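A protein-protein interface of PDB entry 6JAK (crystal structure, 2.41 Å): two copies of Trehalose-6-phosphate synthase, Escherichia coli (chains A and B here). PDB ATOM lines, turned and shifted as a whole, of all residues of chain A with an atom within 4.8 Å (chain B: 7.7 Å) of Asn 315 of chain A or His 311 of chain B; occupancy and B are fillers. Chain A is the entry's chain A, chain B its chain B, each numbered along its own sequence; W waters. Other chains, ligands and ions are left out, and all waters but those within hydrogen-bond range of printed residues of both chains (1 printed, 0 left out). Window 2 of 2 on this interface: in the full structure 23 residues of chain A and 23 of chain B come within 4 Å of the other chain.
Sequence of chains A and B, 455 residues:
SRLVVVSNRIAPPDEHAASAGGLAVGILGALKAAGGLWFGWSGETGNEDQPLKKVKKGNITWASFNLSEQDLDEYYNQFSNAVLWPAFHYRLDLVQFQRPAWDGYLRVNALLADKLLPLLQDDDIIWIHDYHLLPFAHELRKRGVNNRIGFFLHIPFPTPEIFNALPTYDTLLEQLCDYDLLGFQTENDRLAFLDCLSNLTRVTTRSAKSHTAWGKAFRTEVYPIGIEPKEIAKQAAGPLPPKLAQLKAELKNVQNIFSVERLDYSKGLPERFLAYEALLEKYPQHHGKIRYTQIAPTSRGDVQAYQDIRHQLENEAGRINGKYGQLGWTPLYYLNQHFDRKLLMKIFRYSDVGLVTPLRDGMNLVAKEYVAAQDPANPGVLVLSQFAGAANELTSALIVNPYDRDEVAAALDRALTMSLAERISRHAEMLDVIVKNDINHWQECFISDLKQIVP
OD1 of Asn 315 of chain B sits at hydrogen-bond distance from NE2 of His 311 of chain A (3.2 Å). The side-chain amide oxygen (OD1) of Asn 315 of chain A sits close to the backbone carbonyl oxygen (O) of His 311 of chain B (3.2 Å). The backbone carbonyl oxygen (O) of Glu 314 of chain A sits close to the backbone carbonyl oxygen (O) of Glu 314 of chain B, 3.3 Å away.
The guanidinium group of Arg 310 of chain B is in salt-bridge range of the side-chain carboxylate of Glu 314 of chain B (3.5 Å). OE1 of Glu 316 of chain A lies within salt-bridge range of NH2 of Arg 319 of chain A (2.9 Å). The side-chain amide nitrogen (ND2) of Asn 315 of chain B sits at hydrogen-bond distance from the side-chain carboxylate (OE2) of Glu 316 of chain B. OE1 of Glu 316 of chain B is in salt-bridge range of NH2 of Arg 319 of chain B, at 2.8 Å.
Among the printed residues, pairs that only touch across the chains: Glu 314 of chain A with Asn 315 of chain B (3.8 Å), Glu 314 of chain A with Gly 318 of chain B (3.3 Å), Glu 314 of chain A with Arg 319 of chain B (3.5 Å), Asn 315 of chain A with Glu 314 of chain B (3.8 Å), Asn 315 of chain A with Asn 315 of chain B (3.9 Å), Gly 318 of chain A with Glu 314 of chain B (3.4 Å), Gly 318 of chain A with Tyr 334 of chain B (3.8 Å) and Arg 319 of chain A with Glu 314 of chain B (3.5 Å).
Of the printed residues of chain B, Glu 314 of chain A touches Glu 314 (3.3 Å), Asn 315 (3.8 Å), Gly 318 (3.3 Å) and Arg 319 (3.5 Å). Asn 315 of chain A touches just these residues of chain B: His 311, Glu 314 and Asn 315. Gln 307 of chain B touches none of the printed residues of chain A. Ile 309 of chain B touches none of the printed residues of chain A. Of the printed residues of chain A, Glu 314 of chain B touches Glu 314 (3.3 Å), Asn 315 (3.8 Å), Gly 318 (3.4 Å) and Arg 319 (3.5 Å). Of the printed residues of chain A, Asn 315 of chain B touches His 311, Glu 314 and Asn 315. Of the printed residues of chain A, Tyr 334 of chain B touches Gly 318. The nearest residue of chain A that does not touch His 311 of chain B is His 311 of chain A (4.5 Å).
Of the 16 printed residues of chain B, 6 touch a printed residue of chain A. Printed residues of chain B that touch a printed residue of chain A: His 311, Glu 314, Asn 315, Gly 318, Arg 319 and Tyr 334. Hydrophobic or aromatic side chains of chain A that line the printed part of chain B: His 311. Among the printed residues, 11 pairs touch across the chains. Among the printed residues, no Asp or Glu carboxylate lies within 4 Å of a Lys or Arg side-chain nitrogen of the other chain.
His 311 of chain A touches Asn 315 of chain B, and with the chains exchanged Asn 315 of chain A touches His 311 of chain B. Glu 314 of chain B touches its own counterpart, Glu 314 of chain A. Glu 314 of chain A touches Gly 318 of chain B, and with the chains exchanged Gly 318 of chain A touches Glu 314 of chain B. Glu 314 of chain A touches Arg 319 of chain B, and with the chains exchanged Arg 319 of chain A touches Glu 314 of chain B.
Water W1 bridges the side-chain carboxylate of Glu 314 of chain B and the backbone carbonyl oxygen of Arg 319 of chain A.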
ATOM      1  N   HIS A 311     -31.056 -24.094  25.960  1.00  0.00           N
ATOM      2  CA  HIS A 311     -29.840 -23.347  25.669  1.00  0.00           C
ATOM      3  C   HIS A 311     -28.610 -24.243  25.838  1.00  0.00           C
ATOM      4  O   HIS A 311     -27.691 -24.212  25.018  1.00  0.00           O
ATOM      5  CB  HIS A 311     -29.767 -22.115  26.587  1.00  0.00           C
ATOM      6  CG  HIS A 311     -28.760 -21.096  26.151  1.00  0.00           C
ATOM      7  ND1 HIS A 311     -27.443 -21.127  26.567  1.00  0.00           N
ATOM      8  CD2 HIS A 311     -28.877 -20.004  25.355  1.00  0.00           C
ATOM      9  CE1 HIS A 311     -26.785 -20.117  26.021  1.00  0.00           C
ATOM     10  NE2 HIS A 311     -27.634 -19.412  25.290  1.00  0.00           N
ATOM     11  N   GLN A 312     -28.618 -25.107  26.854  1.00  0.00           N
ATOM     12  CA  GLN A 312     -27.461 -25.938  27.136  1.00  0.00           C
ATOM     13  C   GLN A 312     -27.271 -27.010  26.068  1.00  0.00           C
ATOM     14  O   GLN A 312     -26.140 -27.284  25.653  1.00  0.00           O
ATOM     15  CB  GLN A 312     -27.641 -26.556  28.528  1.00  0.00           C
ATOM     16  CG  GLN A 312     -26.422 -27.139  29.169  1.00  0.00           C
ATOM     17  CD  GLN A 312     -26.691 -27.563  30.607  1.00  0.00           C
ATOM     18  OE1 GLN A 312     -27.764 -27.287  31.153  1.00  0.00           O
ATOM     19  NE2 GLN A 312     -25.730 -28.268  31.219  1.00  0.00           N
ATOM     20  N   LEU A 313     -28.373 -27.561  25.552  1.00  0.00           N
ATOM     21  CA  LEU A 313     -28.323 -28.593  24.516  1.00  0.00           C
ATOM     22  C   LEU A 313     -27.896 -28.013  23.180  1.00  0.00           C
ATOM     23  O   LEU A 313     -27.096 -28.623  22.451  1.00  0.00           O
ATOM     24  CB  LEU A 313     -29.701 -29.225  24.345  1.00  0.00           C
ATOM     25  CG  LEU A 313     -30.238 -30.045  25.500  1.00  0.00           C
ATOM     26  CD1 LEU A 313     -31.587 -30.636  25.126  1.00  0.00           C
ATOM     27  CD2 LEU A 313     -29.212 -31.128  25.807  1.00  0.00           C
ATOM     28  N   GLU A 314     -28.448 -26.845  22.836  1.00  0.00           N
ATOM     29  CA  GLU A 314     -28.055 -26.168  21.621  1.00  0.00           C
ATOM     30  C   GLU A 314     -26.569 -25.933  21.609  1.00  0.00           C
ATOM     31  O   GLU A 314     -25.914 -26.105  20.574  1.00  0.00           O
ATOM     32  CB  GLU A 314     -28.795 -24.837  21.479  1.00  0.00           C
ATOM     33  CG  GLU A 314     -30.260 -24.990  21.217  1.00  0.00           C
ATOM     34  CD  GLU A 314     -31.004 -23.661  21.334  1.00  0.00           C
ATOM     35  OE1 GLU A 314     -32.108 -23.571  20.739  1.00  0.00           O
ATOM     36  OE2 GLU A 314     -30.455 -22.700  21.954  1.00  0.00           O
ATOM     37  N   ASN A 315     -26.027 -25.528  22.751  1.00  0.00           N
ATOM     38  CA  ASN A 315     -24.606 -25.274  22.832  1.00  0.00           C
ATOM     39  C   ASN A 315     -23.812 -26.562  22.653  1.00  0.00           C
ATOM     40  O   ASN A 315     -22.834 -26.601  21.892  1.00  0.00           O
ATOM     41  CB  ASN A 315     -24.295 -24.601  24.157  1.00  0.00           C
ATOM     42  CG  ASN A 315     -22.915 -24.082  24.195  1.00  0.00           C
ATOM     43  OD1 ASN A 315     -22.676 -22.925  23.813  1.00  0.00           O
ATOM     44  ND2 ASN A 315     -21.960 -24.945  24.581  1.00  0.00           N
ATOM     45  N   GLU A 316     -24.258 -27.643  23.286  1.00  0.00           N
ATOM     46  CA  GLU A 316     -23.483 -28.865  23.230  1.00  0.00           C
ATOM     47  C   GLU A 316     -23.633 -29.543  21.888  1.00  0.00           C
ATOM     48  O   GLU A 316     -22.680 -30.157  21.407  1.00  0.00           O
ATOM     49  CB  GLU A 316     -23.900 -29.816  24.354  1.00  0.00           C
ATOM     50  CG  GLU A 316     -23.487 -29.354  25.736  1.00  0.00           C
ATOM     51  CD  GLU A 316     -22.243 -30.054  26.256  1.00  0.00           C
ATOM     52  OE1 GLU A 316     -21.126 -29.713  25.809  1.00  0.00           O
ATOM     53  OE2 GLU A 316     -22.409 -30.952  27.126  1.00  0.00           O
ATOM     54  N   ALA A 317     -24.794 -29.406  21.248  1.00  0.00           N
ATOM     55  CA  ALA A 317     -24.923 -29.892  19.885  1.00  0.00           C
ATOM     56  C   ALA A 317     -23.921 -29.160  18.997  1.00  0.00           C
ATOM     57  O   ALA A 317     -23.120 -29.779  18.281  1.00  0.00           O
ATOM     58  CB  ALA A 317     -26.371 -29.712  19.387  1.00  0.00           C
ATOM     59  N   GLY A 318     -23.897 -27.835  19.092  1.00  0.00           N
ATOM     60  CA  GLY A 318     -22.927 -27.087  18.321  1.00  0.00           C
ATOM     61  C   GLY A 318     -21.497 -27.472  18.643  1.00  0.00           C
ATOM     62  O   GLY A 318     -20.666 -27.600  17.745  1.00  0.00           O
ATOM     63  N   ARG A 319     -21.198 -27.714  19.921  1.00  0.00           N
ATOM     64  CA  ARG A 319     -19.806 -27.957  20.267  1.00  0.00           C
ATOM     65  C   ARG A 319     -19.352 -29.331  19.788  1.00  0.00           C
ATOM     66  O   ARG A 319     -18.243 -29.480  19.248  1.00  0.00           O
ATOM     67  CB  ARG A 319     -19.589 -27.801  21.771  1.00  0.00           C
ATOM     68  CG  ARG A 319     -18.178 -28.092  22.191  1.00  0.00           C
ATOM     69  CD  ARG A 319     -18.004 -28.073  23.694  1.00  0.00           C
ATOM     70  NE  ARG A 319     -18.659 -29.193  24.344  1.00  0.00           N
ATOM     71  CZ  ARG A 319     -18.163 -30.419  24.442  1.00  0.00           C
ATOM     72  NH1 ARG A 319     -16.964 -30.706  23.937  1.00  0.00           N
ATOM     73  NH2 ARG A 319     -18.883 -31.371  25.041  1.00  0.00           N
ATOM     74  N   LEU B 263     -11.808 -16.795  14.485  1.00  0.00           N
ATOM     75  CA  LEU B 263     -12.816 -16.248  15.392  1.00  0.00           C
ATOM     76  C   LEU B 263     -12.371 -14.900  15.935  1.00  0.00           C
ATOM     77  O   LEU B 263     -11.340 -14.803  16.605  1.00  0.00           O
ATOM     78  CB  LEU B 263     -13.140 -17.193  16.540  1.00  0.00           C
ATOM     79  CG  LEU B 263     -13.668 -18.500  16.002  1.00  0.00           C
ATOM     80  CD1 LEU B 263     -14.464 -19.240  17.032  1.00  0.00           C
ATOM     81  CD2 LEU B 263     -14.464 -18.262  14.771  1.00  0.00           C
ATOM     82  N   TYR B 306     -11.456 -14.792  22.579  1.00  0.00           N
ATOM     83  CA  TYR B 306     -12.199 -15.258  21.416  1.00  0.00           C
ATOM     84  C   TYR B 306     -13.140 -16.442  21.679  1.00  0.00           C
ATOM     85  O   TYR B 306     -13.872 -16.836  20.773  1.00  0.00           O
ATOM     86  CB  TYR B 306     -11.215 -15.643  20.294  1.00  0.00           C
ATOM     87  CG  TYR B 306     -10.250 -14.534  19.859  1.00  0.00           C
ATOM     88  CD1 TYR B 306     -10.666 -13.203  19.754  1.00  0.00           C
ATOM     89  CD2 TYR B 306      -8.912 -14.819  19.588  1.00  0.00           C
ATOM     90  CE1 TYR B 306      -9.778 -12.193  19.374  1.00  0.00           C
ATOM     91  CE2 TYR B 306      -8.013 -13.813  19.206  1.00  0.00           C
ATOM     92  CZ  TYR B 306      -8.451 -12.502  19.101  1.00  0.00           C
ATOM     93  OH  TYR B 306      -7.557 -11.507  18.721  1.00  0.00           O
ATOM     94  N   GLN B 307     -13.150 -17.025  22.863  1.00  0.00           N
ATOM     95  CA  GLN B 307     -14.003 -18.175  23.159  1.00  0.00           C
ATOM     96  C   GLN B 307     -15.464 -17.825  23.393  1.00  0.00           C
ATOM     97  O   GLN B 307     -16.306 -18.729  23.352  1.00  0.00           O
ATOM     98  CB  GLN B 307     -13.494 -18.805  24.438  1.00  0.00           C
ATOM     99  CG  GLN B 307     -14.026 -18.033  25.708  1.00  0.00           C
ATOM    100  CD  GLN B 307     -13.659 -16.609  25.794  1.00  0.00           C
ATOM    101  OE1 GLN B 307     -13.660 -15.830  24.837  1.00  0.00           O
ATOM    102  NE2 GLN B 307     -13.521 -16.170  26.984  1.00  0.00           N
ATOM    103  N   ASP B 308     -15.752 -16.577  23.775  1.00  0.00           N
ATOM    104  CA  ASP B 308     -17.127 -16.147  23.947  1.00  0.00           C
ATOM    105  C   ASP B 308     -17.765 -16.020  22.585  1.00  0.00           C
ATOM    106  O   ASP B 308     -18.953 -16.299  22.425  1.00  0.00           O
ATOM    107  CB  ASP B 308     -17.229 -14.821  24.715  1.00  0.00           C
ATOM    108  CG  ASP B 308     -16.400 -14.795  26.016  1.00  0.00           C
ATOM    109  OD1 ASP B 308     -16.542 -15.724  26.850  1.00  0.00           O
ATOM    110  OD2 ASP B 308     -15.614 -13.830  26.214  1.00  0.00           O
ATOM    111  N   ILE B 309     -16.964 -15.663  21.585  1.00  0.00           N
ATOM    112  CA  ILE B 309     -17.425 -15.773  20.213  1.00  0.00           C
ATOM    113  C   ILE B 309     -17.635 -17.233  19.866  1.00  0.00           C
ATOM    114  O   ILE B 309     -18.611 -17.595  19.201  1.00  0.00           O
ATOM    115  CB  ILE B 309     -16.422 -15.138  19.246  1.00  0.00           C
ATOM    116  CG1 ILE B 309     -16.340 -13.635  19.484  1.00  0.00           C
ATOM    117  CG2 ILE B 309     -16.810 -15.480  17.795  1.00  0.00           C
ATOM    118  CD1 ILE B 309     -15.215 -13.011  18.756  1.00  0.00           C
ATOM    119  N   ARG B 310     -16.718 -18.095  20.294  1.00  0.00           N
ATOM    120  CA  ARG B 310     -16.869 -19.499  19.957  1.00  0.00           C
ATOM    121  C   ARG B 310     -18.109 -20.091  20.622  1.00  0.00           C
ATOM    122  O   ARG B 310     -18.895 -20.797  19.982  1.00  0.00           O
ATOM    123  CB  ARG B 310     -15.614 -20.237  20.362  1.00  0.00           C
ATOM    124  CG  ARG B 310     -15.427 -21.508  19.596  1.00  0.00           C
ATOM    125  CD  ARG B 310     -15.788 -22.700  20.372  1.00  0.00           C
ATOM    126  NE  ARG B 310     -15.101 -22.781  21.635  1.00  0.00           N
ATOM    127  CZ  ARG B 310     -13.926 -23.363  21.805  1.00  0.00           C
ATOM    128  NH1 ARG B 310     -13.401 -23.376  23.020  1.00  0.00           N
ATOM    129  NH2 ARG B 310     -13.280 -23.936  20.788  1.00  0.00           N
ATOM    130  N   HIS B 311     -18.338 -19.735  21.883  1.00  0.00           N
ATOM    131  CA  HIS B 311     -19.514 -20.175  22.621  1.00  0.00           C
ATOM    132  C   HIS B 311     -20.812 -19.742  21.935  1.00  0.00           C
ATOM    133  O   HIS B 311     -21.790 -20.511  21.871  1.00  0.00           O
ATOM    134  CB  HIS B 311     -19.432 -19.606  24.045  1.00  0.00           C
ATOM    135  CG  HIS B 311     -20.405 -20.209  25.001  1.00  0.00           C
ATOM    136  ND1 HIS B 311     -21.655 -19.668  25.233  1.00  0.00           N
ATOM    137  CD2 HIS B 311     -20.322 -21.314  25.777  1.00  0.00           C
ATOM    138  CE1 HIS B 311     -22.300 -20.407  26.118  1.00  0.00           C
ATOM    139  NE2 HIS B 311     -21.514 -21.415  26.461  1.00  0.00           N
ATOM    140  N   GLN B 312     -20.836 -18.514  21.412  1.00  0.00           N
ATOM    141  CA  GLN B 312     -22.047 -18.006  20.791  1.00  0.00           C
ATOM    142  C   GLN B 312     -22.333 -18.718  19.484  1.00  0.00           C
ATOM    143  O   GLN B 312     -23.493 -19.012  19.176  1.00  0.00           O
ATOM    144  CB  GLN B 312     -21.921 -16.502  20.538  1.00  0.00           C
ATOM    145  CG  GLN B 312     -23.251 -15.874  20.143  1.00  0.00           C
ATOM    146  CD  GLN B 312     -23.212 -14.353  20.019  1.00  0.00           C
ATOM    147  OE1 GLN B 312     -22.215 -13.695  20.371  1.00  0.00           O
ATOM    148  NE2 GLN B 312     -24.303 -13.784  19.489  1.00  0.00           N
ATOM    149  N   LEU B 313     -21.277 -19.054  18.726  1.00  0.00           N
ATOM    150  CA  LEU B 313     -21.477 -19.722  17.453  1.00  0.00           C
ATOM    151  C   LEU B 313     -21.953 -21.146  17.653  1.00  0.00           C
ATOM    152  O   LEU B 313     -22.832 -21.611  16.920  1.00  0.00           O
ATOM    153  CB  LEU B 313     -20.195 -19.714  16.602  1.00  0.00           C
ATOM    154  CG  LEU B 313     -19.659 -18.417  15.999  1.00  0.00           C
ATOM    155  CD1 LEU B 313     -18.494 -18.719  15.044  1.00  0.00           C
ATOM    156  CD2 LEU B 313     -20.757 -17.594  15.304  1.00  0.00           C
ATOM    157  N   GLU B 314     -21.370 -21.863  18.622  1.00  0.00           N
ATOM    158  CA  GLU B 314     -21.857 -23.195  18.942  1.00  0.00           C
ATOM    159  C   GLU B 314     -23.330 -23.148  19.299  1.00  0.00           C
ATOM    160  O   GLU B 314     -24.136 -23.933  18.773  1.00  0.00           O
ATOM    161  CB  GLU B 314     -21.034 -23.808  20.076  1.00  0.00           C
ATOM    162  CG  GLU B 314     -19.582 -24.072  19.685  1.00  0.00           C
ATOM    163  CD  GLU B 314     -18.687 -24.451  20.850  1.00  0.00           C
ATOM    164  OE1 GLU B 314     -17.594 -24.985  20.580  1.00  0.00           O
ATOM    165  OE2 GLU B 314     -19.070 -24.246  22.028  1.00  0.00           O
ATOM    166  N   ASN B 315     -23.716 -22.158  20.096  1.00  0.00           N
ATOM    167  CA  ASN B 315     -25.115 -22.017  20.453  1.00  0.00           C
ATOM    168  C   ASN B 315     -25.966 -21.744  19.217  1.00  0.00           C
ATOM    169  O   ASN B 315     -27.060 -22.306  19.076  1.00  0.00           O
ATOM    170  CB  ASN B 315     -25.277 -20.908  21.490  1.00  0.00           C
ATOM    171  CG  ASN B 315     -26.683 -20.817  22.020  1.00  0.00           C
ATOM    172  OD1 ASN B 315     -27.042 -21.504  22.990  1.00  0.00           O
ATOM    173  ND2 ASN B 315     -27.500 -19.971  21.391  1.00  0.00           N
ATOM    174  N   GLU B 316     -25.483 -20.898  18.296  1.00  0.00           N
ATOM    175  CA  GLU B 316     -26.332 -20.573  17.162  1.00  0.00           C
ATOM    176  C   GLU B 316     -26.379 -21.703  16.145  1.00  0.00           C
ATOM    177  O   GLU B 316     -27.435 -21.940  15.556  1.00  0.00           O
ATOM    178  CB  GLU B 316     -25.901 -19.255  16.514  1.00  0.00           C
ATOM    179  CG  GLU B 316     -26.196 -18.103  17.450  1.00  0.00           C
ATOM    180  CD  GLU B 316     -27.709 -17.909  17.674  1.00  0.00           C
ATOM    181  OE1 GLU B 316     -28.350 -17.207  16.865  1.00  0.00           O
ATOM    182  OE2 GLU B 316     -28.243 -18.443  18.684  1.00  0.00           O
ATOM    183  N   ALA B 317     -25.301 -22.472  15.997  1.00  0.00           N
ATOM    184  CA  ALA B 317     -25.381 -23.674  15.177  1.00  0.00           C
ATOM    185  C   ALA B 317     -26.458 -24.600  15.713  1.00  0.00           C
ATOM    186  O   ALA B 317     -27.395 -24.976  14.991  1.00  0.00           O
ATOM    187  CB  ALA B 317     -24.036 -24.397  15.158  1.00  0.00           C
ATOM    188  N   GLY B 318     -26.399 -24.881  17.011  1.00  0.00           N
ATOM    189  CA  GLY B 318     -27.398 -25.742  17.616  1.00  0.00           C
ATOM    190  C   GLY B 318     -28.809 -25.215  17.475  1.00  0.00           C
ATOM    191  O   GLY B 318     -29.747 -25.985  17.266  1.00  0.00           O
ATOM    192  N   ARG B 319     -28.987 -23.907  17.591  1.00  0.00           N
ATOM    193  CA  ARG B 319     -30.355 -23.392  17.584  1.00  0.00           C
ATOM    194  C   ARG B 319     -30.941 -23.442  16.177  1.00  0.00           C
ATOM    195  O   ARG B 319     -32.110 -23.802  15.991  1.00  0.00           O
ATOM    196  CB  ARG B 319     -30.406 -21.976  18.168  1.00  0.00           C
ATOM    197  CG  ARG B 319     -31.790 -21.330  18.088  1.00  0.00           C
ATOM    198  CD  ARG B 319     -31.799 -19.866  18.505  1.00  0.00           C
ATOM    199  NE  ARG B 319     -31.096 -18.988  17.558  1.00  0.00           N
ATOM    200  CZ  ARG B 319     -31.576 -18.530  16.396  1.00  0.00           C
ATOM    201  NH1 ARG B 319     -32.793 -18.843  15.947  1.00  0.00           N
ATOM    202  NH2 ARG B 319     -30.813 -17.749  15.657  1.00  0.00           N
ATOM    203  N   TYR B 334     -20.908 -26.497  11.120  1.00  0.00           N
ATOM    204  CA  TYR B 334     -19.952 -25.622  11.806  1.00  0.00           C
ATOM    205  C   TYR B 334     -18.768 -26.460  12.238  1.00  0.00           C
ATOM    206  O   TYR B 334     -18.948 -27.485  12.909  1.00  0.00           O
ATOM    207  CB  TYR B 334     -20.606 -24.925  12.997  1.00  0.00           C
ATOM    208  CG  TYR B 334     -19.645 -24.352  14.019  1.00  0.00           C
ATOM    209  CD1 TYR B 334     -18.778 -23.329  13.683  1.00  0.00           C
ATOM    210  CD2 TYR B 334     -19.629 -24.823  15.349  1.00  0.00           C
ATOM    211  CE1 TYR B 334     -17.898 -22.791  14.624  1.00  0.00           C
ATOM    212  CE2 TYR B 334     -18.754 -24.291  16.294  1.00  0.00           C
ATOM    213  CZ  TYR B 334     -17.892 -23.266  15.924  1.00  0.00           C
ATOM    214  OH  TYR B 334     -16.999 -22.699  16.814  1.00  0.00           O
HETATM  215  O   HOH W   1     -16.233 -27.066  18.913  1.00  0.00           O
